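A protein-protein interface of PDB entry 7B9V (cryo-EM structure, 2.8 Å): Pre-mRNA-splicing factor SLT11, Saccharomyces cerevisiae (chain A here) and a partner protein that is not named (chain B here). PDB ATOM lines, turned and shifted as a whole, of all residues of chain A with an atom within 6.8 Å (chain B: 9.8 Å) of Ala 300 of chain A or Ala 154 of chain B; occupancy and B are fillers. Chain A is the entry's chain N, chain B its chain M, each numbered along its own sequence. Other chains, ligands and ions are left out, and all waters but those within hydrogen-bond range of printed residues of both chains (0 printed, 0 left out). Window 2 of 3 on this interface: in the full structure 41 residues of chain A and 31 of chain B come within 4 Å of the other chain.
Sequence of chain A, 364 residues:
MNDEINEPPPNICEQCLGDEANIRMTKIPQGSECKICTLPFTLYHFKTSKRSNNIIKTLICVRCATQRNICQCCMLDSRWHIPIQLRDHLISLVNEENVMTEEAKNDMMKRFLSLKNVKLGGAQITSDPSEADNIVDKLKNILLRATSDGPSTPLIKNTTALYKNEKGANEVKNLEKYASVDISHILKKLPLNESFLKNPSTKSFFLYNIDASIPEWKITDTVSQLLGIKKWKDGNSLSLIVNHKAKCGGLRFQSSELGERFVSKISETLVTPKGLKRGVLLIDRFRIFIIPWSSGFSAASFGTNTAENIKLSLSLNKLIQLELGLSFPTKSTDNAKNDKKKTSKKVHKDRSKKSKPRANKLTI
Among the printed residues, pairs that only touch across the chains: Ile 241 of chain A with Arg 161 of chain B (3.7 Å), Ala 299 of chain A with Ala 154 of chain B (3.6 Å), Ala 300 of chain A with Ala 154 of chain B (3.7 Å) and Thr 304 of chain A with Pro 153 of chain B (3.3 Å).
Of the 19 printed residues of chain B, 3 touch a printed residue of chain A.
Printed residues of chain B that touch a printed residue of chain A: Pro 153, Ala 154 and Arg 161.
Of the 12 printed residues of chain A, 4 touch a printed residue of chain B.
Printed residues of chain A that touch a printed residue of chain B: Ile 241, Ala 299, Ala 300 and Thr 304.
Hydrophobic or aromatic side chains of chain A that line the printed part of chain B: Ile 241, Ala 299 and Ala 300.
Among the printed residues, 4 pairs touch across the chains.
Among the printed residues, no Asp or Glu carboxylate lies within 4 Å of a Lys or Arg side-chain nitrogen of the other chain.
The guanidinium group (NE) of Arg 161 of chain B lies within salt-bridge range of the side-chain carboxylate (OE2) of Glu 157 of chain B (3.0 Å).
NH2 of Arg 161 of chain B lies within hydrogen-bond range of O of Ile 173 of chain B, 3.4 Å away.
The side-chain hydroxyl of Thr 304 of chain A lies within hydrogen-bond range of the side-chain carboxylate of Glu 308 of chain A.
Of the printed residues of chain B, Ile 241 of chain A touches Arg 161 (3.7 Å).
Of the printed residues of chain B, Ala 299 of chain A touches Ala 154 (3.6 Å).
Ala 300 of chain A touches just one residue of chain B: Ala 154.
Phe 302 of chain A touches none of the printed residues of chain B.
Printed residues of chain B within 4 Å of Thr 304 of chain A: Pro 153 (3.3 Å).
Of the printed residues of chain A, Pro 153 of chain B touches Thr 304 (3.3 Å).
Of chain A, only Ala 299 and Ala 300 come within 4 Å of Ala 154 of chain B.
Printed residues of chain A within 4 Å of Arg 161 of chain B: Ile 241 (3.7 Å).
Asn 180 of chain B touches none of the printed residues of chain A.
The nearest residue of chain B that does not touch Ala 300 of chain A is Gln 155 of chain B (6.0 Å).
The nearest printed residue of chain A that does not touch Ala 154 of chain B is Thr 304 of chain A (4.8 Å).
The nearest printed residue of chain A that does not touch Arg 161 of chain B is Ala 299 of chain A (4.9 Å).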
ATOM      1  N   ILE A 186      18.068 -42.077 -10.607  1.00  0.00           N
ATOM      2  CA  ILE A 186      18.280 -40.754 -10.004  1.00  0.00           C
ATOM      3  C   ILE A 186      18.848 -40.799  -8.584  1.00  0.00           C
ATOM      4  O   ILE A 186      19.402 -39.798  -8.121  1.00  0.00           O
ATOM      5  CB  ILE A 186      16.974 -39.920 -10.062  1.00  0.00           C
ATOM      6  CG1 ILE A 186      15.869 -40.462  -9.142  1.00  0.00           C
ATOM      7  CG2 ILE A 186      16.494 -39.759 -11.504  1.00  0.00           C
ATOM      8  CD1 ILE A 186      14.561 -39.657  -9.222  1.00  0.00           C
ATOM      9  N   LYS A 189      22.189 -39.755  -8.817  1.00  0.00           N
ATOM     10  CA  LYS A 189      22.295 -38.313  -9.040  1.00  0.00           C
ATOM     11  C   LYS A 189      22.120 -37.532  -7.739  1.00  0.00           C
ATOM     12  O   LYS A 189      22.782 -36.511  -7.524  1.00  0.00           O
ATOM     13  CB  LYS A 189      21.263 -37.863 -10.075  1.00  0.00           C
ATOM     14  CG  LYS A 189      21.519 -38.378 -11.497  1.00  0.00           C
ATOM     15  CD  LYS A 189      20.453 -37.870 -12.472  1.00  0.00           C
ATOM     16  CE  LYS A 189      20.749 -38.275 -13.913  1.00  0.00           C
ATOM     17  NZ  LYS A 189      21.834 -37.464 -14.529  1.00  0.00           N
ATOM     18  N   ILE A 241      14.909 -24.847  -4.708  1.00  0.00           N
ATOM     19  CA  ILE A 241      13.865 -25.674  -5.299  1.00  0.00           C
ATOM     20  C   ILE A 241      13.443 -26.672  -4.235  1.00  0.00           C
ATOM     21  O   ILE A 241      14.301 -27.286  -3.601  1.00  0.00           O
ATOM     22  CB  ILE A 241      14.344 -26.384  -6.578  1.00  0.00           C
ATOM     23  CG1 ILE A 241      14.756 -25.352  -7.638  1.00  0.00           C
ATOM     24  CG2 ILE A 241      13.271 -27.330  -7.111  1.00  0.00           C
ATOM     25  CD1 ILE A 241      15.245 -25.964  -8.919  1.00  0.00           C
ATOM     26  N   PHE A 297      22.393 -29.340  -9.416  1.00  0.00           N
ATOM     27  CA  PHE A 297      21.025 -29.822  -9.511  1.00  0.00           C
ATOM     28  C   PHE A 297      20.164 -28.918 -10.379  1.00  0.00           C
ATOM     29  O   PHE A 297      20.508 -27.775 -10.683  1.00  0.00           O
ATOM     30  CB  PHE A 297      20.382 -29.957  -8.126  1.00  0.00           C
ATOM     31  CG  PHE A 297      20.139 -28.653  -7.415  1.00  0.00           C
ATOM     32  CD1 PHE A 297      21.135 -28.086  -6.639  1.00  0.00           C
ATOM     33  CD2 PHE A 297      18.877 -28.052  -7.433  1.00  0.00           C
ATOM     34  CE1 PHE A 297      20.915 -26.901  -5.970  1.00  0.00           C
ATOM     35  CE2 PHE A 297      18.650 -26.871  -6.767  1.00  0.00           C
ATOM     36  CZ  PHE A 297      19.674 -26.294  -6.034  1.00  0.00           C
ATOM     37  N   SER A 298      19.017 -29.464 -10.757  1.00  0.00           N
ATOM     38  CA  SER A 298      17.936 -28.704 -11.360  1.00  0.00           C
ATOM     39  C   SER A 298      16.631 -29.339 -10.911  1.00  0.00           C
ATOM     40  O   SER A 298      16.622 -30.237 -10.064  1.00  0.00           O
ATOM     41  CB  SER A 298      18.046 -28.668 -12.881  1.00  0.00           C
ATOM     42  OG  SER A 298      18.019 -29.976 -13.427  1.00  0.00           O
ATOM     43  N   ALA A 299      15.520 -28.802 -11.431  1.00  0.00           N
ATOM     44  CA  ALA A 299      14.191 -29.325 -11.114  1.00  0.00           C
ATOM     45  C   ALA A 299      14.017 -30.779 -11.550  1.00  0.00           C
ATOM     46  O   ALA A 299      13.187 -31.497 -10.980  1.00  0.00           O
ATOM     47  CB  ALA A 299      13.117 -28.450 -11.756  1.00  0.00           C
ATOM     48  N   ALA A 300      14.765 -31.227 -12.573  1.00  0.00           N
ATOM     49  CA  ALA A 300      14.676 -32.603 -13.054  1.00  0.00           C
ATOM     50  C   ALA A 300      15.186 -33.639 -12.062  1.00  0.00           C
ATOM     51  O   ALA A 300      14.945 -34.830 -12.284  1.00  0.00           O
ATOM     52  CB  ALA A 300      15.440 -32.733 -14.372  1.00  0.00           C
ATOM     53  N   SER A 301      15.925 -33.212 -11.021  1.00  0.00           N
ATOM     54  CA  SER A 301      16.558 -34.117 -10.063  1.00  0.00           C
ATOM     55  C   SER A 301      15.548 -34.976  -9.309  1.00  0.00           C
ATOM     56  O   SER A 301      15.878 -36.082  -8.866  1.00  0.00           O
ATOM     57  CB  SER A 301      17.376 -33.321  -9.046  1.00  0.00           C
ATOM     58  OG  SER A 301      18.195 -32.338  -9.650  1.00  0.00           O
ATOM     59  N   PHE A 302      14.324 -34.479  -9.143  1.00  0.00           N
ATOM     60  CA  PHE A 302      13.344 -35.139  -8.302  1.00  0.00           C
ATOM     61  C   PHE A 302      12.276 -35.888  -9.088  1.00  0.00           C
ATOM     62  O   PHE A 302      11.341 -36.423  -8.483  1.00  0.00           O
ATOM     63  CB  PHE A 302      12.708 -34.091  -7.392  1.00  0.00           C
ATOM     64  CG  PHE A 302      13.708 -33.104  -6.848  1.00  0.00           C
ATOM     65  CD1 PHE A 302      14.548 -33.456  -5.810  1.00  0.00           C
ATOM     66  CD2 PHE A 302      13.786 -31.813  -7.363  1.00  0.00           C
ATOM     67  CE1 PHE A 302      15.470 -32.561  -5.306  1.00  0.00           C
ATOM     68  CE2 PHE A 302      14.705 -30.907  -6.864  1.00  0.00           C
ATOM     69  CZ  PHE A 302      15.548 -31.286  -5.837  1.00  0.00           C
ATOM     70  N   GLY A 303      12.435 -36.014 -10.400  1.00  0.00           N
ATOM     71  CA  GLY A 303      11.507 -36.774 -11.210  1.00  0.00           C
ATOM     72  C   GLY A 303      10.802 -35.910 -12.238  1.00  0.00           C
ATOM     73  O   GLY A 303      10.553 -34.726 -11.994  1.00  0.00           O
ATOM     74  N   THR A 304      10.463 -36.494 -13.387  1.00  0.00           N
ATOM     75  CA  THR A 304       9.856 -35.756 -14.490  1.00  0.00           C
ATOM     76  C   THR A 304       8.335 -35.682 -14.406  1.00  0.00           C
ATOM     77  O   THR A 304       7.745 -34.782 -15.012  1.00  0.00           O
ATOM     78  CB  THR A 304      10.254 -36.375 -15.834  1.00  0.00           C
ATOM     79  OG1 THR A 304       9.665 -37.676 -15.952  1.00  0.00           O
ATOM     80  CG2 THR A 304      11.767 -36.504 -15.932  1.00  0.00           C
ATOM     81  N   GLU A 308       6.698 -40.237 -10.417  1.00  0.00           N
ATOM     82  CA  GLU A 308       8.118 -40.367 -10.108  1.00  0.00           C
ATOM     83  C   GLU A 308       8.463 -39.647  -8.811  1.00  0.00           C
ATOM     84  O   GLU A 308       9.273 -40.142  -8.017  1.00  0.00           O
ATOM     85  CB  GLU A 308       8.966 -39.844 -11.265  1.00  0.00           C
ATOM     86  CG  GLU A 308       9.004 -40.778 -12.465  1.00  0.00           C
ATOM     87  CD  GLU A 308       9.839 -40.231 -13.597  1.00  0.00           C
ATOM     88  OE1 GLU A 308       9.823 -39.003 -13.789  1.00  0.00           O
ATOM     89  OE2 GLU A 308      10.509 -41.024 -14.291  1.00  0.00           O
ATOM     90  N   LEU B 146       5.555 -20.323 -24.848  1.00  0.00           N
ATOM     91  CA  LEU B 146       6.801 -20.820 -25.380  1.00  0.00           C
ATOM     92  C   LEU B 146       6.808 -20.847 -26.896  1.00  0.00           C
ATOM     93  O   LEU B 146       7.753 -21.391 -27.454  1.00  0.00           O
ATOM     94  CB  LEU B 146       7.083 -22.218 -24.827  1.00  0.00           C
ATOM     95  CG  LEU B 146       7.249 -22.330 -23.314  1.00  0.00           C
ATOM     96  CD1 LEU B 146       7.069 -23.761 -22.849  1.00  0.00           C
ATOM     97  CD2 LEU B 146       8.627 -21.832 -22.954  1.00  0.00           C
ATOM     98  N   LEU B 151       9.297 -28.639 -24.868  1.00  0.00           N
ATOM     99  CA  LEU B 151      10.112 -28.473 -23.680  1.00  0.00           C
ATOM    100  C   LEU B 151       9.710 -29.535 -22.674  1.00  0.00           C
ATOM    101  O   LEU B 151       8.534 -29.887 -22.577  1.00  0.00           O
ATOM    102  CB  LEU B 151       9.945 -27.071 -23.086  1.00  0.00           C
ATOM    103  CG  LEU B 151      11.185 -26.455 -22.443  1.00  0.00           C
ATOM    104  CD1 LEU B 151      12.155 -25.980 -23.508  1.00  0.00           C
ATOM    105  CD2 LEU B 151      10.802 -25.308 -21.528  1.00  0.00           C
ATOM    106  N   LYS B 152      10.696 -30.045 -21.939  1.00  0.00           N
ATOM    107  CA  LYS B 152      10.440 -31.096 -20.967  1.00  0.00           C
ATOM    108  C   LYS B 152       9.703 -30.505 -19.759  1.00  0.00           C
ATOM    109  O   LYS B 152       9.764 -29.292 -19.545  1.00  0.00           O
ATOM    110  CB  LYS B 152      11.763 -31.761 -20.557  1.00  0.00           C
ATOM    111  CG  LYS B 152      12.364 -32.644 -21.636  1.00  0.00           C
ATOM    112  CD  LYS B 152      13.816 -32.970 -21.370  1.00  0.00           C
ATOM    113  CE  LYS B 152      14.363 -33.838 -22.484  1.00  0.00           C
ATOM    114  NZ  LYS B 152      15.825 -34.057 -22.361  1.00  0.00           N
ATOM    115  N   PRO B 153       8.906 -31.322 -19.025  1.00  0.00           N
ATOM    116  CA  PRO B 153       8.087 -30.755 -17.924  1.00  0.00           C
ATOM    117  C   PRO B 153       8.888 -30.118 -16.799  1.00  0.00           C
ATOM    118  O   PRO B 153       8.476 -29.072 -16.272  1.00  0.00           O
ATOM    119  CB  PRO B 153       7.273 -31.958 -17.441  1.00  0.00           C
ATOM    120  CG  PRO B 153       8.004 -33.144 -17.898  1.00  0.00           C
ATOM    121  CD  PRO B 153       8.637 -32.769 -19.187  1.00  0.00           C
ATOM    122  N   ALA B 154       9.984 -30.754 -16.382  1.00  0.00           N
ATOM    123  CA  ALA B 154      10.839 -30.175 -15.355  1.00  0.00           C
ATOM    124  C   ALA B 154      11.483 -28.875 -15.831  1.00  0.00           C
ATOM    125  O   ALA B 154      11.729 -27.975 -15.020  1.00  0.00           O
ATOM    126  CB  ALA B 154      11.905 -31.182 -14.973  1.00  0.00           C
ATOM    127  N   GLN B 155      11.775 -28.774 -17.135  1.00  0.00           N
ATOM    128  CA  GLN B 155      12.310 -27.541 -17.710  1.00  0.00           C
ATOM    129  C   GLN B 155      11.288 -26.408 -17.624  1.00  0.00           C
ATOM    130  O   GLN B 155      11.643 -25.256 -17.315  1.00  0.00           O
ATOM    131  CB  GLN B 155      12.711 -27.811 -19.159  1.00  0.00           C
ATOM    132  CG  GLN B 155      13.829 -26.963 -19.714  1.00  0.00           C
ATOM    133  CD  GLN B 155      14.391 -27.553 -20.990  1.00  0.00           C
ATOM    134  OE1 GLN B 155      13.790 -28.443 -21.592  1.00  0.00           O
ATOM    135  NE2 GLN B 155      15.548 -27.060 -21.413  1.00  0.00           N
ATOM    136  N   ILE B 156      10.019 -26.723 -17.937  1.00  0.00           N
ATOM    137  CA  ILE B 156       8.924 -25.761 -17.818  1.00  0.00           C
ATOM    138  C   ILE B 156       8.781 -25.311 -16.371  1.00  0.00           C
ATOM    139  O   ILE B 156       8.587 -24.114 -16.088  1.00  0.00           O
ATOM    140  CB  ILE B 156       7.617 -26.371 -18.369  1.00  0.00           C
ATOM    141  CG1 ILE B 156       7.734 -26.648 -19.869  1.00  0.00           C
ATOM    142  CG2 ILE B 156       6.419 -25.502 -18.080  1.00  0.00           C
ATOM    143  CD1 ILE B 156       6.561 -27.399 -20.457  1.00  0.00           C
ATOM    144  N   GLU B 157       8.857 -26.279 -15.438  1.00  0.00           N
ATOM    145  CA  GLU B 157       8.760 -25.967 -14.017  1.00  0.00           C
ATOM    146  C   GLU B 157       9.898 -25.062 -13.579  1.00  0.00           C
ATOM    147  O   GLU B 157       9.676 -24.149 -12.787  1.00  0.00           O
ATOM    148  CB  GLU B 157       8.750 -27.248 -13.184  1.00  0.00           C
ATOM    149  CG  GLU B 157       8.371 -27.018 -11.718  1.00  0.00           C
ATOM    150  CD  GLU B 157       8.637 -28.223 -10.842  1.00  0.00           C
ATOM    151  OE1 GLU B 157       8.888 -29.312 -11.395  1.00  0.00           O
ATOM    152  OE2 GLU B 157       8.605 -28.079  -9.601  1.00  0.00           O
ATOM    153  N   SER B 158      11.119 -25.305 -14.089  1.00  0.00           N
ATOM    154  CA  SER B 158      12.260 -24.460 -13.745  1.00  0.00           C
ATOM    155  C   SER B 158      12.065 -23.032 -14.248  1.00  0.00           C
ATOM    156  O   SER B 158      12.465 -22.074 -13.570  1.00  0.00           O
ATOM    157  CB  SER B 158      13.559 -25.048 -14.301  1.00  0.00           C
ATOM    158  OG  SER B 158      13.625 -24.923 -15.710  1.00  0.00           O
ATOM    159  N   ARG B 159      11.484 -22.875 -15.457  1.00  0.00           N
ATOM    160  CA  ARG B 159      11.178 -21.531 -15.964  1.00  0.00           C
ATOM    161  C   ARG B 159      10.180 -20.801 -15.078  1.00  0.00           C
ATOM    162  O   ARG B 159      10.376 -19.618 -14.739  1.00  0.00           O
ATOM    163  CB  ARG B 159      10.601 -21.610 -17.389  1.00  0.00           C
ATOM    164  CG  ARG B 159      11.634 -21.857 -18.426  1.00  0.00           C
ATOM    165  CD  ARG B 159      11.331 -21.939 -19.892  1.00  0.00           C
ATOM    166  NE  ARG B 159      12.550 -22.308 -20.617  1.00  0.00           N
ATOM    167  CZ  ARG B 159      12.866 -21.869 -21.828  1.00  0.00           C
ATOM    168  NH1 ARG B 159      12.080 -21.034 -22.486  1.00  0.00           N
ATOM    169  NH2 ARG B 159      13.983 -22.304 -22.402  1.00  0.00           N
ATOM    170  N   ILE B 160       9.080 -21.498 -14.732  1.00  0.00           N
ATOM    171  CA  ILE B 160       8.032 -20.914 -13.897  1.00  0.00           C
ATOM    172  C   ILE B 160       8.588 -20.583 -12.521  1.00  0.00           C
ATOM    173  O   ILE B 160       8.235 -19.558 -11.922  1.00  0.00           O
ATOM    174  CB  ILE B 160       6.813 -21.861 -13.843  1.00  0.00           C
ATOM    175  CG1 ILE B 160       6.180 -21.963 -15.224  1.00  0.00           C
ATOM    176  CG2 ILE B 160       5.736 -21.400 -12.866  1.00  0.00           C
ATOM    177  CD1 ILE B 160       5.174 -23.075 -15.345  1.00  0.00           C
ATOM    178  N   ARG B 161       9.482 -21.452 -12.012  1.00  0.00           N
ATOM    179  CA  ARG B 161      10.150 -21.216 -10.740  1.00  0.00           C
ATOM    180  C   ARG B 161      10.987 -19.958 -10.788  1.00  0.00           C
ATOM    181  O   ARG B 161      11.027 -19.224  -9.806  1.00  0.00           O
ATOM    182  CB  ARG B 161      11.001 -22.410 -10.324  1.00  0.00           C
ATOM    183  CG  ARG B 161      10.200 -23.518  -9.681  1.00  0.00           C
ATOM    184  CD  ARG B 161      11.064 -24.696  -9.282  1.00  0.00           C
ATOM    185  NE  ARG B 161      10.276 -25.739  -8.634  1.00  0.00           N
ATOM    186  CZ  ARG B 161       9.858 -25.720  -7.376  1.00  0.00           C
ATOM    187  NH1 ARG B 161      10.135 -24.712  -6.565  1.00  0.00           N
ATOM    188  NH2 ARG B 161       9.129 -26.734  -6.922  1.00  0.00           N
ATOM    189  N   PHE B 162      11.721 -19.741 -11.894  1.00  0.00           N
ATOM    190  CA  PHE B 162      12.564 -18.553 -11.993  1.00  0.00           C
ATOM    191  C   PHE B 162      11.724 -17.282 -11.975  1.00  0.00           C
ATOM    192  O   PHE B 162      11.989 -16.373 -11.181  1.00  0.00           O
ATOM    193  CB  PHE B 162      13.461 -18.577 -13.233  1.00  0.00           C
ATOM    194  CG  PHE B 162      14.487 -17.447 -13.254  1.00  0.00           C
ATOM    195  CD1 PHE B 162      15.711 -17.611 -12.621  1.00  0.00           C
ATOM    196  CD2 PHE B 162      14.225 -16.224 -13.879  1.00  0.00           C
ATOM    197  CE1 PHE B 162      16.650 -16.589 -12.607  1.00  0.00           C
ATOM    198  CE2 PHE B 162      15.155 -15.196 -13.855  1.00  0.00           C
ATOM    199  CZ  PHE B 162      16.370 -15.383 -13.232  1.00  0.00           C
ATOM    200  N   ILE B 173       5.269 -24.198  -5.547  1.00  0.00           N
ATOM    201  CA  ILE B 173       5.078 -24.271  -6.989  1.00  0.00           C
ATOM    202  C   ILE B 173       4.957 -25.746  -7.358  1.00  0.00           C
ATOM    203  O   ILE B 173       5.751 -26.575  -6.899  1.00  0.00           O
ATOM    204  CB  ILE B 173       6.220 -23.572  -7.762  1.00  0.00           C
ATOM    205  CG1 ILE B 173       6.183 -22.059  -7.519  1.00  0.00           C
ATOM    206  CG2 ILE B 173       6.187 -23.847  -9.268  1.00  0.00           C
ATOM    207  CD1 ILE B 173       7.275 -21.297  -8.223  1.00  0.00           C
ATOM    208  N   ARG B 174       3.957 -26.067  -8.179  1.00  0.00           N
ATOM    209  CA  ARG B 174       3.784 -27.389  -8.750  1.00  0.00           C
ATOM    210  C   ARG B 174       3.399 -27.225 -10.212  1.00  0.00           C
ATOM    211  O   ARG B 174       2.642 -26.317 -10.566  1.00  0.00           O
ATOM    212  CB  ARG B 174       2.691 -28.185  -7.999  1.00  0.00           C
ATOM    213  CG  ARG B 174       2.507 -29.616  -8.489  1.00  0.00           C
ATOM    214  CD  ARG B 174       1.436 -30.399  -7.782  1.00  0.00           C
ATOM    215  NE  ARG B 174       1.268 -31.676  -8.467  1.00  0.00           N
ATOM    216  CZ  ARG B 174       0.119 -32.324  -8.576  1.00  0.00           C
ATOM    217  NH1 ARG B 174      -0.995 -31.841  -8.057  1.00  0.00           N
ATOM    218  NH2 ARG B 174       0.088 -33.481  -9.230  1.00  0.00           N
ATOM    219  N   TYR B 175       3.932 -28.106 -11.054  1.00  0.00           N
ATOM    220  CA  TYR B 175       3.571 -28.207 -12.454  1.00  0.00           C
ATOM    221  C   TYR B 175       2.937 -29.570 -12.689  1.00  0.00           C
ATOM    222  O   TYR B 175       3.436 -30.593 -12.206  1.00  0.00           O
ATOM    223  CB  TYR B 175       4.785 -28.018 -13.366  1.00  0.00           C
ATOM    224  CG  TYR B 175       4.434 -28.005 -14.831  1.00  0.00           C
ATOM    225  CD1 TYR B 175       3.683 -26.969 -15.372  1.00  0.00           C
ATOM    226  CD2 TYR B 175       4.853 -29.029 -15.677  1.00  0.00           C
ATOM    227  CE1 TYR B 175       3.358 -26.950 -16.709  1.00  0.00           C
ATOM    228  CE2 TYR B 175       4.532 -29.016 -17.023  1.00  0.00           C
ATOM    229  CZ  TYR B 175       3.784 -27.971 -17.530  1.00  0.00           C
ATOM    230  OH  TYR B 175       3.453 -27.940 -18.863  1.00  0.00           O
ATOM    231  N   VAL B 176       1.839 -29.568 -13.434  1.00  0.00           N
ATOM    232  CA  VAL B 176       1.045 -30.749 -13.745  1.00  0.00           C
ATOM    233  C   VAL B 176       1.236 -31.012 -15.229  1.00  0.00           C
ATOM    234  O   VAL B 176       0.844 -30.186 -16.053  1.00  0.00           O
ATOM    235  CB  VAL B 176      -0.437 -30.540 -13.404  1.00  0.00           C
ATOM    236  CG1 VAL B 176      -1.218 -31.815 -13.643  1.00  0.00           C
ATOM    237  CG2 VAL B 176      -0.582 -30.086 -11.967  1.00  0.00           C
ATOM    238  N   GLU B 177       1.857 -32.149 -15.575  1.00  0.00           N
ATOM    239  CA  GLU B 177       2.158 -32.443 -16.977  1.00  0.00           C
ATOM    240  C   GLU B 177       0.904 -32.789 -17.776  1.00  0.00           C
ATOM    241  O   GLU B 177       0.789 -32.390 -18.944  1.00  0.00           O
ATOM    242  CB  GLU B 177       3.169 -33.588 -17.054  1.00  0.00           C
ATOM    243  CG  GLU B 177       3.653 -33.924 -18.461  1.00  0.00           C
ATOM    244  CD  GLU B 177       4.622 -35.085 -18.488  1.00  0.00           C
ATOM    245  OE1 GLU B 177       4.523 -35.964 -17.605  1.00  0.00           O
ATOM    246  OE2 GLU B 177       5.477 -35.128 -19.397  1.00  0.00           O
ATOM    247  N   ASN B 180      -0.926 -29.765 -18.232  1.00  0.00           N
ATOM    248  CA  ASN B 180       0.016 -28.793 -18.839  1.00  0.00           C
ATOM    249  C   ASN B 180      -0.204 -27.390 -18.266  1.00  0.00           C
ATOM    250  O   ASN B 180      -0.314 -26.392 -18.985  1.00  0.00           O
ATOM    251  CB  ASN B 180      -0.060 -28.811 -20.374  1.00  0.00           C
ATOM    252  CG  ASN B 180       1.185 -28.239 -21.028  1.00  0.00           C
ATOM    253  OD1 ASN B 180       2.158 -28.953 -21.261  1.00  0.00           O
ATOM    254  ND2 ASN B 180       1.164 -26.942 -21.319  1.00  0.00           N
